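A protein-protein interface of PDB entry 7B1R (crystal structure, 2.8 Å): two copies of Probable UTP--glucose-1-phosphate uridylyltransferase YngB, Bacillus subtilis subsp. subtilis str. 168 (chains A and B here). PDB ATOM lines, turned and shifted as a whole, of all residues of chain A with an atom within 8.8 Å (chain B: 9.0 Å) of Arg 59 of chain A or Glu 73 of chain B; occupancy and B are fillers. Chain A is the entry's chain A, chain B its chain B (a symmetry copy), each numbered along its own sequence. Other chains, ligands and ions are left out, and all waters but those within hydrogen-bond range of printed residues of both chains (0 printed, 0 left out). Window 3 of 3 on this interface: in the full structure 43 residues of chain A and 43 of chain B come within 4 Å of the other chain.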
ATOM      1  N   ALA A  11      -5.678  12.952  -0.216  1.00  0.00           N
ATOM      2  CA  ALA A  11      -6.516  12.467  -1.304  1.00  0.00           C
ATOM      3  C   ALA A  11      -6.895  11.010  -1.067  1.00  0.00           C
ATOM      4  O   ALA A  11      -6.527  10.161  -1.882  1.00  0.00           O
ATOM      5  CB  ALA A  11      -5.760  12.573  -2.599  1.00  0.00           C
ATOM      6  N   ALA A  12      -7.639  10.732   0.018  1.00  0.00           N
ATOM      7  CA  ALA A  12      -7.937   9.342   0.310  1.00  0.00           C
ATOM      8  C   ALA A  12      -9.433   9.073   0.506  1.00  0.00           C
ATOM      9  O   ALA A  12      -9.801   7.990   0.960  1.00  0.00           O
ATOM     10  CB  ALA A  12      -7.100   8.877   1.472  1.00  0.00           C
ATOM     11  N   GLY A  13     -10.299  10.013   0.097  1.00  0.00           N
ATOM     12  CA  GLY A  13     -11.749   9.826   0.116  1.00  0.00           C
ATOM     13  C   GLY A  13     -12.251   8.746  -0.841  1.00  0.00           C
ATOM     14  O   GLY A  13     -11.536   8.333  -1.752  1.00  0.00           O
ATOM     15  N   LEU A  14     -13.488   8.291  -0.612  1.00  0.00           N
ATOM     16  CA  LEU A  14     -14.172   7.385  -1.520  1.00  0.00           C
ATOM     17  C   LEU A  14     -15.138   8.176  -2.398  1.00  0.00           C
ATOM     18  O   LEU A  14     -15.749   7.607  -3.291  1.00  0.00           O
ATOM     19  CB  LEU A  14     -14.904   6.322  -0.699  1.00  0.00           C
ATOM     20  CG  LEU A  14     -14.314   4.915  -0.762  1.00  0.00           C
ATOM     21  CD1 LEU A  14     -13.137   4.769   0.177  1.00  0.00           C
ATOM     22  CD2 LEU A  14     -15.370   3.877  -0.415  1.00  0.00           C
ATOM     23  N   THR A  16     -18.149   9.829  -2.078  1.00  0.00           N
ATOM     24  CA  THR A  16     -19.512   9.340  -2.140  1.00  0.00           C
ATOM     25  C   THR A  16     -20.419  10.334  -2.859  1.00  0.00           C
ATOM     26  O   THR A  16     -21.325   9.939  -3.581  1.00  0.00           O
ATOM     27  CB  THR A  16     -19.953   8.933  -0.741  1.00  0.00           C
ATOM     28  OG1 THR A  16     -19.071   7.818  -0.571  1.00  0.00           O
ATOM     29  CG2 THR A  16     -21.420   8.563  -0.678  1.00  0.00           C
ATOM     30  N   LYS A  23     -17.506   5.100  -8.502  1.00  0.00           N
ATOM     31  CA  LYS A  23     -17.616   3.752  -7.969  1.00  0.00           C
ATOM     32  C   LYS A  23     -16.239   3.091  -8.011  1.00  0.00           C
ATOM     33  O   LYS A  23     -15.802   2.510  -7.033  1.00  0.00           O
ATOM     34  CB  LYS A  23     -18.712   2.953  -8.693  1.00  0.00           C
ATOM     35  CG  LYS A  23     -18.844   1.491  -8.270  1.00  0.00           C
ATOM     36  CD  LYS A  23     -20.213   0.911  -8.643  1.00  0.00           C
ATOM     37  CE  LYS A  23     -20.412  -0.547  -8.286  1.00  0.00           C
ATOM     38  NZ  LYS A  23     -19.213  -1.359  -8.605  1.00  0.00           N
ATOM     39  N   ALA A  24     -15.556   3.191  -9.153  1.00  0.00           N
ATOM     40  CA  ALA A  24     -14.368   2.381  -9.362  1.00  0.00           C
ATOM     41  C   ALA A  24     -13.220   3.269  -9.809  1.00  0.00           C
ATOM     42  O   ALA A  24     -12.229   2.775 -10.338  1.00  0.00           O
ATOM     43  CB  ALA A  24     -14.615   1.291 -10.392  1.00  0.00           C
ATOM     44  N   GLN A  25     -13.383   4.578  -9.641  1.00  0.00           N
ATOM     45  CA  GLN A  25     -12.323   5.484 -10.023  1.00  0.00           C
ATOM     46  C   GLN A  25     -12.348   6.701  -9.100  1.00  0.00           C
ATOM     47  O   GLN A  25     -13.406   7.091  -8.615  1.00  0.00           O
ATOM     48  CB  GLN A  25     -12.472   5.807 -11.504  1.00  0.00           C
ATOM     49  CG  GLN A  25     -13.714   6.609 -11.806  1.00  0.00           C
ATOM     50  CD  GLN A  25     -13.750   6.936 -13.278  1.00  0.00           C
ATOM     51  OE1 GLN A  25     -12.897   6.460 -14.050  1.00  0.00           O
ATOM     52  NE2 GLN A  25     -14.739   7.748 -13.660  1.00  0.00           N
ATOM     53  N   PRO A  26     -11.192   7.341  -8.824  1.00  0.00           N
ATOM     54  CA  PRO A  26     -11.091   8.353  -7.776  1.00  0.00           C
ATOM     55  C   PRO A  26     -11.748   9.678  -8.097  1.00  0.00           C
ATOM     56  O   PRO A  26     -11.716  10.150  -9.232  1.00  0.00           O
ATOM     57  CB  PRO A  26      -9.593   8.644  -7.644  1.00  0.00           C
ATOM     58  CG  PRO A  26      -8.947   7.467  -8.351  1.00  0.00           C
ATOM     59  CD  PRO A  26      -9.906   7.088  -9.469  1.00  0.00           C
ATOM     60  N   GLU A  28     -10.655  12.592  -7.364  1.00  0.00           N
ATOM     61  CA  GLU A  28      -9.701  13.607  -7.790  1.00  0.00           C
ATOM     62  C   GLU A  28      -9.382  13.473  -9.283  1.00  0.00           C
ATOM     63  O   GLU A  28      -8.878  14.404  -9.922  1.00  0.00           O
ATOM     64  CB  GLU A  28      -8.498  13.749  -6.857  1.00  0.00           C
ATOM     65  CG  GLU A  28      -8.202  12.516  -6.043  1.00  0.00           C
ATOM     66  CD  GLU A  28      -9.143  12.193  -4.890  1.00  0.00           C
ATOM     67  OE1 GLU A  28      -8.949  12.736  -3.766  1.00  0.00           O
ATOM     68  OE2 GLU A  28     -10.052  11.376  -5.112  1.00  0.00           O
ATOM     69  N   ILE A  56      -1.176  12.092  -0.087  1.00  0.00           N
ATOM     70  CA  ILE A  56      -1.541  11.020   0.826  1.00  0.00           C
ATOM     71  C   ILE A  56      -2.720  10.307   0.184  1.00  0.00           C
ATOM     72  O   ILE A  56      -3.838  10.823   0.169  1.00  0.00           O
ATOM     73  CB  ILE A  56      -1.992  11.585   2.179  1.00  0.00           C
ATOM     74  CG1 ILE A  56      -1.184  12.799   2.649  1.00  0.00           C
ATOM     75  CG2 ILE A  56      -2.069  10.484   3.205  1.00  0.00           C
ATOM     76  CD1 ILE A  56       0.263  12.539   2.984  1.00  0.00           C
ATOM     77  N   THR A  57      -2.456   9.126  -0.348  1.00  0.00           N
ATOM     78  CA  THR A  57      -3.408   8.447  -1.201  1.00  0.00           C
ATOM     79  C   THR A  57      -3.979   7.237  -0.455  1.00  0.00           C
ATOM     80  O   THR A  57      -3.500   6.871   0.617  1.00  0.00           O
ATOM     81  CB  THR A  57      -2.703   8.079  -2.513  1.00  0.00           C
ATOM     82  OG1 THR A  57      -3.657   7.603  -3.458  1.00  0.00           O
ATOM     83  CG2 THR A  57      -1.662   6.995  -2.332  1.00  0.00           C
ATOM     84  N   GLY A  58      -5.011   6.626  -1.044  1.00  0.00           N
ATOM     85  CA  GLY A  58      -5.616   5.411  -0.532  1.00  0.00           C
ATOM     86  C   GLY A  58      -5.442   4.252  -1.512  1.00  0.00           C
ATOM     87  O   GLY A  58      -4.540   4.281  -2.351  1.00  0.00           O
ATOM     88  N   ARG A  59      -6.328   3.246  -1.379  1.00  0.00           N
ATOM     89  CA  ARG A  59      -6.398   2.078  -2.244  1.00  0.00           C
ATOM     90  C   ARG A  59      -7.079   2.426  -3.570  1.00  0.00           C
ATOM     91  O   ARG A  59      -7.986   3.272  -3.646  1.00  0.00           O
ATOM     92  CB  ARG A  59      -7.118   0.932  -1.530  1.00  0.00           C
ATOM     93  CG  ARG A  59      -6.228   0.077  -0.638  1.00  0.00           C
ATOM     94  CD  ARG A  59      -7.008  -0.731   0.390  1.00  0.00           C
ATOM     95  NE  ARG A  59      -6.682  -0.394   1.776  1.00  0.00           N
ATOM     96  CZ  ARG A  59      -6.997   0.753   2.388  1.00  0.00           C
ATOM     97  NH1 ARG A  59      -7.648   1.701   1.732  1.00  0.00           N
ATOM     98  NH2 ARG A  59      -6.649   0.964   3.646  1.00  0.00           N
ATOM     99  N   ASN A  60      -6.623   1.724  -4.614  1.00  0.00           N
ATOM    100  CA  ASN A  60      -7.196   1.781  -5.952  1.00  0.00           C
ATOM    101  C   ASN A  60      -7.218   3.224  -6.424  1.00  0.00           C
ATOM    102  O   ASN A  60      -8.174   3.617  -7.072  1.00  0.00           O
ATOM    103  CB  ASN A  60      -8.626   1.223  -6.041  1.00  0.00           C
ATOM    104  CG  ASN A  60      -8.769  -0.197  -5.530  1.00  0.00           C
ATOM    105  OD1 ASN A  60      -9.359  -0.431  -4.474  1.00  0.00           O
ATOM    106  ND2 ASN A  60      -8.227  -1.158  -6.266  1.00  0.00           N
ATOM    107  N   LYS A  61      -6.182   3.994  -6.082  1.00  0.00           N
ATOM    108  CA  LYS A  61      -6.077   5.332  -6.627  1.00  0.00           C
ATOM    109  C   LYS A  61      -4.823   5.456  -7.483  1.00  0.00           C
ATOM    110  O   LYS A  61      -4.235   6.536  -7.518  1.00  0.00           O
ATOM    111  CB  LYS A  61      -6.053   6.377  -5.512  1.00  0.00           C
ATOM    112  CG  LYS A  61      -7.368   6.524  -4.781  1.00  0.00           C
ATOM    113  CD  LYS A  61      -7.511   7.836  -4.063  1.00  0.00           C
ATOM    114  CE  LYS A  61      -8.953   7.987  -3.624  1.00  0.00           C
ATOM    115  NZ  LYS A  61      -9.258   9.375  -3.202  1.00  0.00           N
ATOM    116  N   ARG A  62      -4.433   4.362  -8.158  1.00  0.00           N
ATOM    117  CA  ARG A  62      -3.215   4.357  -8.959  1.00  0.00           C
ATOM    118  C   ARG A  62      -3.325   5.426 -10.031  1.00  0.00           C
ATOM    119  O   ARG A  62      -2.320   6.009 -10.418  1.00  0.00           O
ATOM    120  CB  ARG A  62      -2.961   3.020  -9.674  1.00  0.00           C
ATOM    121  N   SER A  63      -4.544   5.667 -10.530  1.00  0.00           N
ATOM    122  CA  SER A  63      -4.657   6.540 -11.690  1.00  0.00           C
ATOM    123  C   SER A  63      -4.092   7.944 -11.438  1.00  0.00           C
ATOM    124  O   SER A  63      -3.633   8.578 -12.386  1.00  0.00           O
ATOM    125  CB  SER A  63      -6.039   6.552 -12.280  1.00  0.00           C
ATOM    126  OG  SER A  63      -6.984   7.087 -11.372  1.00  0.00           O
ATOM    127  N   ILE A  64      -4.134   8.437 -10.185  1.00  0.00           N
ATOM    128  CA  ILE A  64      -3.518   9.710  -9.847  1.00  0.00           C
ATOM    129  C   ILE A  64      -2.021   9.654 -10.177  1.00  0.00           C
ATOM    130  O   ILE A  64      -1.514  10.523 -10.883  1.00  0.00           O
ATOM    131  CB  ILE A  64      -3.747  10.044  -8.366  1.00  0.00           C
ATOM    132  CG1 ILE A  64      -5.231  10.208  -8.039  1.00  0.00           C
ATOM    133  CG2 ILE A  64      -2.915  11.236  -7.905  1.00  0.00           C
ATOM    134  CD1 ILE A  64      -5.536  10.074  -6.541  1.00  0.00           C
ATOM    135  N   GLU A  65      -1.322   8.635  -9.647  1.00  0.00           N
ATOM    136  CA  GLU A  65       0.113   8.424  -9.800  1.00  0.00           C
ATOM    137  C   GLU A  65       0.461   8.260 -11.285  1.00  0.00           C
ATOM    138  O   GLU A  65       1.489   8.749 -11.750  1.00  0.00           O
ATOM    139  CB  GLU A  65       0.602   7.240  -8.946  1.00  0.00           C
ATOM    140  CG  GLU A  65      -0.179   7.068  -7.644  1.00  0.00           C
ATOM    141  CD  GLU A  65       0.162   5.852  -6.796  1.00  0.00           C
ATOM    142  OE1 GLU A  65       1.169   5.183  -7.139  1.00  0.00           O
ATOM    143  OE2 GLU A  65      -0.580   5.576  -5.798  1.00  0.00           O
ATOM    144  N   ILE A 102       2.326   8.512  -0.247  1.00  0.00           N
ATOM    145  CA  ILE A 102       2.321   7.573   0.867  1.00  0.00           C
ATOM    146  C   ILE A 102       0.897   7.058   0.980  1.00  0.00           C
ATOM    147  O   ILE A 102      -0.041   7.805   0.726  1.00  0.00           O
ATOM    148  CB  ILE A 102       2.715   8.281   2.179  1.00  0.00           C
ATOM    149  CG1 ILE A 102       2.851   7.299   3.341  1.00  0.00           C
ATOM    150  CG2 ILE A 102       1.721   9.376   2.528  1.00  0.00           C
ATOM    151  CD1 ILE A 102       4.257   6.840   3.578  1.00  0.00           C
ATOM    152  N   ARG A 103       0.731   5.815   1.429  1.00  0.00           N
ATOM    153  CA  ARG A 103      -0.622   5.389   1.747  1.00  0.00           C
ATOM    154  C   ARG A 103      -0.984   5.668   3.198  1.00  0.00           C
ATOM    155  O   ARG A 103      -0.273   5.259   4.114  1.00  0.00           O
ATOM    156  CB  ARG A 103      -0.821   3.929   1.380  1.00  0.00           C
ATOM    157  CG  ARG A 103      -1.642   3.830   0.115  1.00  0.00           C
ATOM    158  CD  ARG A 103      -0.899   3.156  -0.996  1.00  0.00           C
ATOM    159  NE  ARG A 103      -1.801   2.043  -1.277  1.00  0.00           N
ATOM    160  CZ  ARG A 103      -1.845   1.362  -2.410  1.00  0.00           C
ATOM    161  NH1 ARG A 103      -1.052   1.690  -3.416  1.00  0.00           N
ATOM    162  NH2 ARG A 103      -2.690   0.357  -2.535  1.00  0.00           N
ATOM    163  N   GLN A 104      -2.095   6.383   3.394  1.00  0.00           N
ATOM    164  CA  GLN A 104      -2.702   6.504   4.711  1.00  0.00           C
ATOM    165  C   GLN A 104      -3.343   5.161   4.973  1.00  0.00           C
ATOM    166  O   GLN A 104      -4.164   4.718   4.179  1.00  0.00           O
ATOM    167  CB  GLN A 104      -3.868   7.468   4.615  1.00  0.00           C
ATOM    168  CG  GLN A 104      -4.083   8.262   5.883  1.00  0.00           C
ATOM    169  CD  GLN A 104      -5.472   8.846   5.868  1.00  0.00           C
ATOM    170  OE1 GLN A 104      -6.344   8.386   5.122  1.00  0.00           O
ATOM    171  NE2 GLN A 104      -5.675   9.857   6.703  1.00  0.00           N
ATOM    172  N   LYS A 105      -2.925   4.471   6.021  1.00  0.00           N
ATOM    173  CA  LYS A 105      -3.261   3.052   6.010  1.00  0.00           C
ATOM    174  C   LYS A 105      -4.733   2.852   6.380  1.00  0.00           C
ATOM    175  O   LYS A 105      -5.421   2.090   5.703  1.00  0.00           O
ATOM    176  CB  LYS A 105      -2.241   2.232   6.812  1.00  0.00           C
ATOM    177  CG  LYS A 105      -0.867   2.076   6.158  1.00  0.00           C
ATOM    178  CD  LYS A 105       0.242   1.775   7.147  1.00  0.00           C
ATOM    179  CE  LYS A 105       0.708   2.970   7.956  1.00  0.00           C
ATOM    180  NZ  LYS A 105       1.644   2.556   9.034  1.00  0.00           N
ATOM    181  N   GLU A 106      -5.190   3.560   7.436  1.00  0.00           N
ATOM    182  CA  GLU A 106      -6.574   3.570   7.902  1.00  0.00           C
ATOM    183  C   GLU A 106      -7.141   4.982   7.809  1.00  0.00           C
ATOM    184  O   GLU A 106      -6.449   5.946   8.135  1.00  0.00           O
ATOM    185  CB  GLU A 106      -6.743   3.039   9.332  1.00  0.00           C
ATOM    186  CG  GLU A 106      -5.819   3.665  10.363  1.00  0.00           C
ATOM    187  CD  GLU A 106      -4.435   3.038  10.439  1.00  0.00           C
ATOM    188  OE1 GLU A 106      -4.348   1.850  10.821  1.00  0.00           O
ATOM    189  OE2 GLU A 106      -3.443   3.732  10.095  1.00  0.00           O
ATOM    190  N   PRO A 107      -8.423   5.136   7.393  1.00  0.00           N
ATOM    191  CA  PRO A 107      -8.971   6.449   7.047  1.00  0.00           C
ATOM    192  C   PRO A 107      -9.405   7.169   8.316  1.00  0.00           C
ATOM    193  O   PRO A 107     -10.451   6.872   8.871  1.00  0.00           O
ATOM    194  CB  PRO A 107     -10.170   6.104   6.152  1.00  0.00           C
ATOM    195  CG  PRO A 107     -10.625   4.739   6.643  1.00  0.00           C
ATOM    196  CD  PRO A 107      -9.415   4.057   7.251  1.00  0.00           C
ATOM    197  N   ARG B  70     -18.748  -5.999  -7.595  1.00  0.00           N
ATOM    198  CA  ARG B  70     -19.042  -5.519  -6.255  1.00  0.00           C
ATOM    199  C   ARG B  70     -17.780  -4.923  -5.620  1.00  0.00           C
ATOM    200  O   ARG B  70     -16.798  -5.636  -5.433  1.00  0.00           O
ATOM    201  CB  ARG B  70     -19.597  -6.695  -5.445  1.00  0.00           C
ATOM    202  CG  ARG B  70     -21.113  -6.697  -5.281  1.00  0.00           C
ATOM    203  CD  ARG B  70     -21.672  -7.496  -4.098  1.00  0.00           C
ATOM    204  NE  ARG B  70     -23.123  -7.378  -4.107  1.00  0.00           N
ATOM    205  CZ  ARG B  70     -23.916  -7.813  -5.098  1.00  0.00           C
ATOM    206  NH1 ARG B  70     -23.408  -8.430  -6.156  1.00  0.00           N
ATOM    207  NH2 ARG B  70     -25.226  -7.633  -5.027  1.00  0.00           N
ATOM    208  N   SER B  71     -17.800  -3.622  -5.282  1.00  0.00           N
ATOM    209  CA  SER B  71     -16.691  -2.989  -4.563  1.00  0.00           C
ATOM    210  C   SER B  71     -16.861  -3.131  -3.044  1.00  0.00           C
ATOM    211  O   SER B  71     -17.639  -2.400  -2.434  1.00  0.00           O
ATOM    212  CB  SER B  71     -16.511  -1.518  -4.939  1.00  0.00           C
ATOM    213  OG  SER B  71     -17.059  -1.204  -6.214  1.00  0.00           O
ATOM    214  N   ALA B  72     -16.105  -4.045  -2.420  1.00  0.00           N
ATOM    215  CA  ALA B  72     -16.331  -4.402  -1.021  1.00  0.00           C
ATOM    216  C   ALA B  72     -16.178  -3.185  -0.111  1.00  0.00           C
ATOM    217  O   ALA B  72     -17.104  -2.858   0.625  1.00  0.00           O
ATOM    218  CB  ALA B  72     -15.433  -5.542  -0.586  1.00  0.00           C
ATOM    219  N   GLU B  73     -15.016  -2.527  -0.191  1.00  0.00           N
ATOM    220  CA  GLU B  73     -14.676  -1.366   0.614  1.00  0.00           C
ATOM    221  C   GLU B  73     -15.738  -0.269   0.505  1.00  0.00           C
ATOM    222  O   GLU B  73     -15.975   0.466   1.462  1.00  0.00           O
ATOM    223  CB  GLU B  73     -13.322  -0.798   0.180  1.00  0.00           C
ATOM    224  CG  GLU B  73     -12.146  -1.260   1.020  1.00  0.00           C
ATOM    225  CD  GLU B  73     -11.172  -0.138   1.346  1.00  0.00           C
ATOM    226  OE1 GLU B  73     -10.001  -0.462   1.653  1.00  0.00           O
ATOM    227  OE2 GLU B  73     -11.584   1.060   1.299  1.00  0.00           O
ATOM    228  N   LEU B  74     -16.340  -0.129  -0.678  1.00  0.00           N
ATOM    229  CA  LEU B  74     -17.334   0.902  -0.913  1.00  0.00           C
ATOM    230  C   LEU B  74     -18.647   0.505  -0.241  1.00  0.00           C
ATOM    231  O   LEU B  74     -19.386   1.367   0.225  1.00  0.00           O
ATOM    232  CB  LEU B  74     -17.534   1.093  -2.423  1.00  0.00           C
ATOM    233  CG  LEU B  74     -18.565   2.161  -2.760  1.00  0.00           C
ATOM    234  CD1 LEU B  74     -18.011   3.554  -2.484  1.00  0.00           C
ATOM    235  CD2 LEU B  74     -19.061   2.019  -4.180  1.00  0.00           C
ATOM    236  N   GLU B  75     -18.951  -0.804  -0.235  1.00  0.00           N
ATOM    237  CA  GLU B  75     -20.204  -1.324   0.305  1.00  0.00           C
ATOM    238  C   GLU B  75     -20.221  -1.139   1.824  1.00  0.00           C
ATOM    239  O   GLU B  75     -21.210  -0.639   2.372  1.00  0.00           O
ATOM    240  CB  GLU B  75     -20.443  -2.774  -0.135  1.00  0.00           C
ATOM    241  N   PHE B  76     -19.113  -1.543   2.475  1.00  0.00           N
ATOM    242  CA  PHE B  76     -18.878  -1.283   3.884  1.00  0.00           C
ATOM    243  C   PHE B  76     -19.119   0.202   4.181  1.00  0.00           C
ATOM    244  O   PHE B  76     -19.986   0.545   4.975  1.00  0.00           O
ATOM    245  CB  PHE B  76     -17.518  -1.832   4.329  1.00  0.00           C
ATOM    246  CG  PHE B  76     -17.149  -1.551   5.770  1.00  0.00           C
ATOM    247  CD1 PHE B  76     -17.760  -2.235   6.818  1.00  0.00           C
ATOM    248  CD2 PHE B  76     -16.183  -0.598   6.091  1.00  0.00           C
ATOM    249  CE1 PHE B  76     -17.416  -1.969   8.141  1.00  0.00           C
ATOM    250  CE2 PHE B  76     -15.840  -0.334   7.413  1.00  0.00           C
ATOM    251  CZ  PHE B  76     -16.461  -1.016   8.438  1.00  0.00           C
ATOM    252  N   ASN B  77     -18.411   1.095   3.486  1.00  0.00           N
ATOM    253  CA  ASN B  77     -18.394   2.505   3.841  1.00  0.00           C
ATOM    254  C   ASN B  77     -19.770   3.138   3.664  1.00  0.00           C
ATOM    255  O   ASN B  77     -20.101   4.119   4.330  1.00  0.00           O
ATOM    256  CB  ASN B  77     -17.377   3.276   3.007  1.00  0.00           C
ATOM    257  CG  ASN B  77     -16.974   4.581   3.649  1.00  0.00           C
ATOM    258  OD1 ASN B  77     -17.440   5.652   3.247  1.00  0.00           O
ATOM    259  ND2 ASN B  77     -16.117   4.483   4.656  1.00  0.00           N
ATOM    260  N   LEU B  78     -20.557   2.582   2.745  1.00  0.00           N
ATOM    261  CA  LEU B  78     -21.872   3.120   2.452  1.00  0.00           C
ATOM    262  C   LEU B  78     -22.847   2.714   3.555  1.00  0.00           C
ATOM    263  O   LEU B  78     -23.705   3.524   3.936  1.00  0.00           O
ATOM    264  CB  LEU B  78     -22.311   2.567   1.099  1.00  0.00           C
ATOM    265  CG  LEU B  78     -21.672   3.235  -0.107  1.00  0.00           C
ATOM    266  CD1 LEU B  78     -22.138   2.515  -1.349  1.00  0.00           C
ATOM    267  CD2 LEU B  78     -22.047   4.706  -0.167  1.00  0.00           C
ATOM    268  N   ARG B  79     -22.699   1.458   4.034  1.00  0.00           N
ATOM    269  CA  ARG B  79     -23.419   0.944   5.195  1.00  0.00           C
ATOM    270  C   ARG B  79     -23.160   1.825   6.424  1.00  0.00           C
ATOM    271  O   ARG B  79     -24.112   2.421   6.934  1.00  0.00           O
ATOM    272  CB  ARG B  79     -23.070  -0.522   5.467  1.00  0.00           C
ATOM    273  CG  ARG B  79     -23.818  -1.151   6.632  1.00  0.00           C
ATOM    274  CD  ARG B  79     -23.472  -2.617   6.744  1.00  0.00           C
ATOM    275  NE  ARG B  79     -23.097  -3.133   5.427  1.00  0.00           N
ATOM    276  CZ  ARG B  79     -23.912  -3.658   4.499  1.00  0.00           C
ATOM    277  NH1 ARG B  79     -23.393  -4.082   3.357  1.00  0.00           N
ATOM    278  NH2 ARG B  79     -25.215  -3.784   4.715  1.00  0.00           N
ATOM    279  N   GLU B  80     -21.885   1.919   6.863  1.00  0.00           N
ATOM    280  CA  GLU B  80     -21.472   2.693   8.022  1.00  0.00           C
ATOM    281  C   GLU B  80     -21.812   4.167   7.869  1.00  0.00           C
ATOM    282  O   GLU B  80     -21.269   4.962   8.621  1.00  0.00           O
ATOM    283  CB  GLU B  80     -19.950   2.706   8.186  1.00  0.00           C
ATOM    284  CG  GLU B  80     -19.289   1.337   8.108  1.00  0.00           C
ATOM    285  CD  GLU B  80     -19.976   0.211   8.886  1.00  0.00           C
ATOM    286  OE1 GLU B  80     -20.776  -0.616   8.246  1.00  0.00           O
ATOM    287  OE2 GLU B  80     -19.714   0.140  10.143  1.00  0.00           O
ATOM    288  N   LEU B  87     -26.147   2.134  -1.415  1.00  0.00           N
ATOM    289  CA  LEU B  87     -25.611   0.784  -1.435  1.00  0.00           C
ATOM    290  C   LEU B  87     -26.458  -0.090  -2.367  1.00  0.00           C
ATOM    291  O   LEU B  87     -25.971  -1.065  -2.928  1.00  0.00           O
ATOM    292  CB  LEU B  87     -25.546   0.227  -0.008  1.00  0.00           C
ATOM    293  CG  LEU B  87     -25.284  -1.285   0.107  1.00  0.00           C
ATOM    294  CD1 LEU B  87     -23.974  -1.717  -0.557  1.00  0.00           C
ATOM    295  CD2 LEU B  87     -25.287  -1.730   1.560  1.00  0.00           C
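Hydrophobic or aromatic side chains of chain B within 4 Å of the printed part of chain A: Leu 74 and Leu 78. Of the 26 printed residues of chain A, 4 touch a printed residue of chain B. Hydrophobic or aromatic side chains of chain A within 4 Å of the printed part of chain B: Leu 14. Among the printed residues, Asp or Glu carboxylates within 4 Å of a Lys or Arg side-chain nitrogen of the other chain: Arg 59 of chain A with Glu 73 of chain B.
NH2 of Arg 59 of chain A sits at hydrogen-bond distance from O of Lys 105 of chain A (2.6 Å).
Glu 73 of chain B touches Leu 14 of chain A. Leu 14 of chain A touches Leu 74 of chain B (CD2 to CD1, 3.4 Å). Thr 16 of chain A touches Leu 78 of chain B.
OE1 of Glu 73 of chain B lies within salt-bridge range of NH1 of Arg 59 of chain A (3.2 Å). The side-chain amino group of Lys 23 of chain A sits at hydrogen-bond distance from the side-chain hydroxyl of Ser 71 of chain B (3.2 Å).
Of the printed residues of chain B, Arg 59 of chain A touches Glu 73 (3.2 Å). Glu 73 of chain B touches just these residues of chain A: Leu 14 (3.9 Å) and Arg 59 (3.2 Å). No residue of chain B comes within 4 Å of Asn 60 of chain A. No residue of chain A comes within 4 Å of Ala 72 of chain B. Of the printed residues of chain A, Ser 71 of chain B touches Lys 23 (3.2 Å). Of the printed residues of chain A, Leu 74 of chain B touches Leu 14 (3.4 Å). Gln 104 of chain A touches none of the printed residues of chain B. The nearest printed residue of chain B that does not touch Arg 59 of chain A is Leu 74 of chain B (9.2 Å). The nearest printed residue of chain A that does not touch Leu 74 of chain B is Lys 23 of chain A (4.1 Å).
No position is printed for both chains. Of the 5 pairs that touch across the chains among the printed residues, none has its exchanged pair printed and touching as well.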
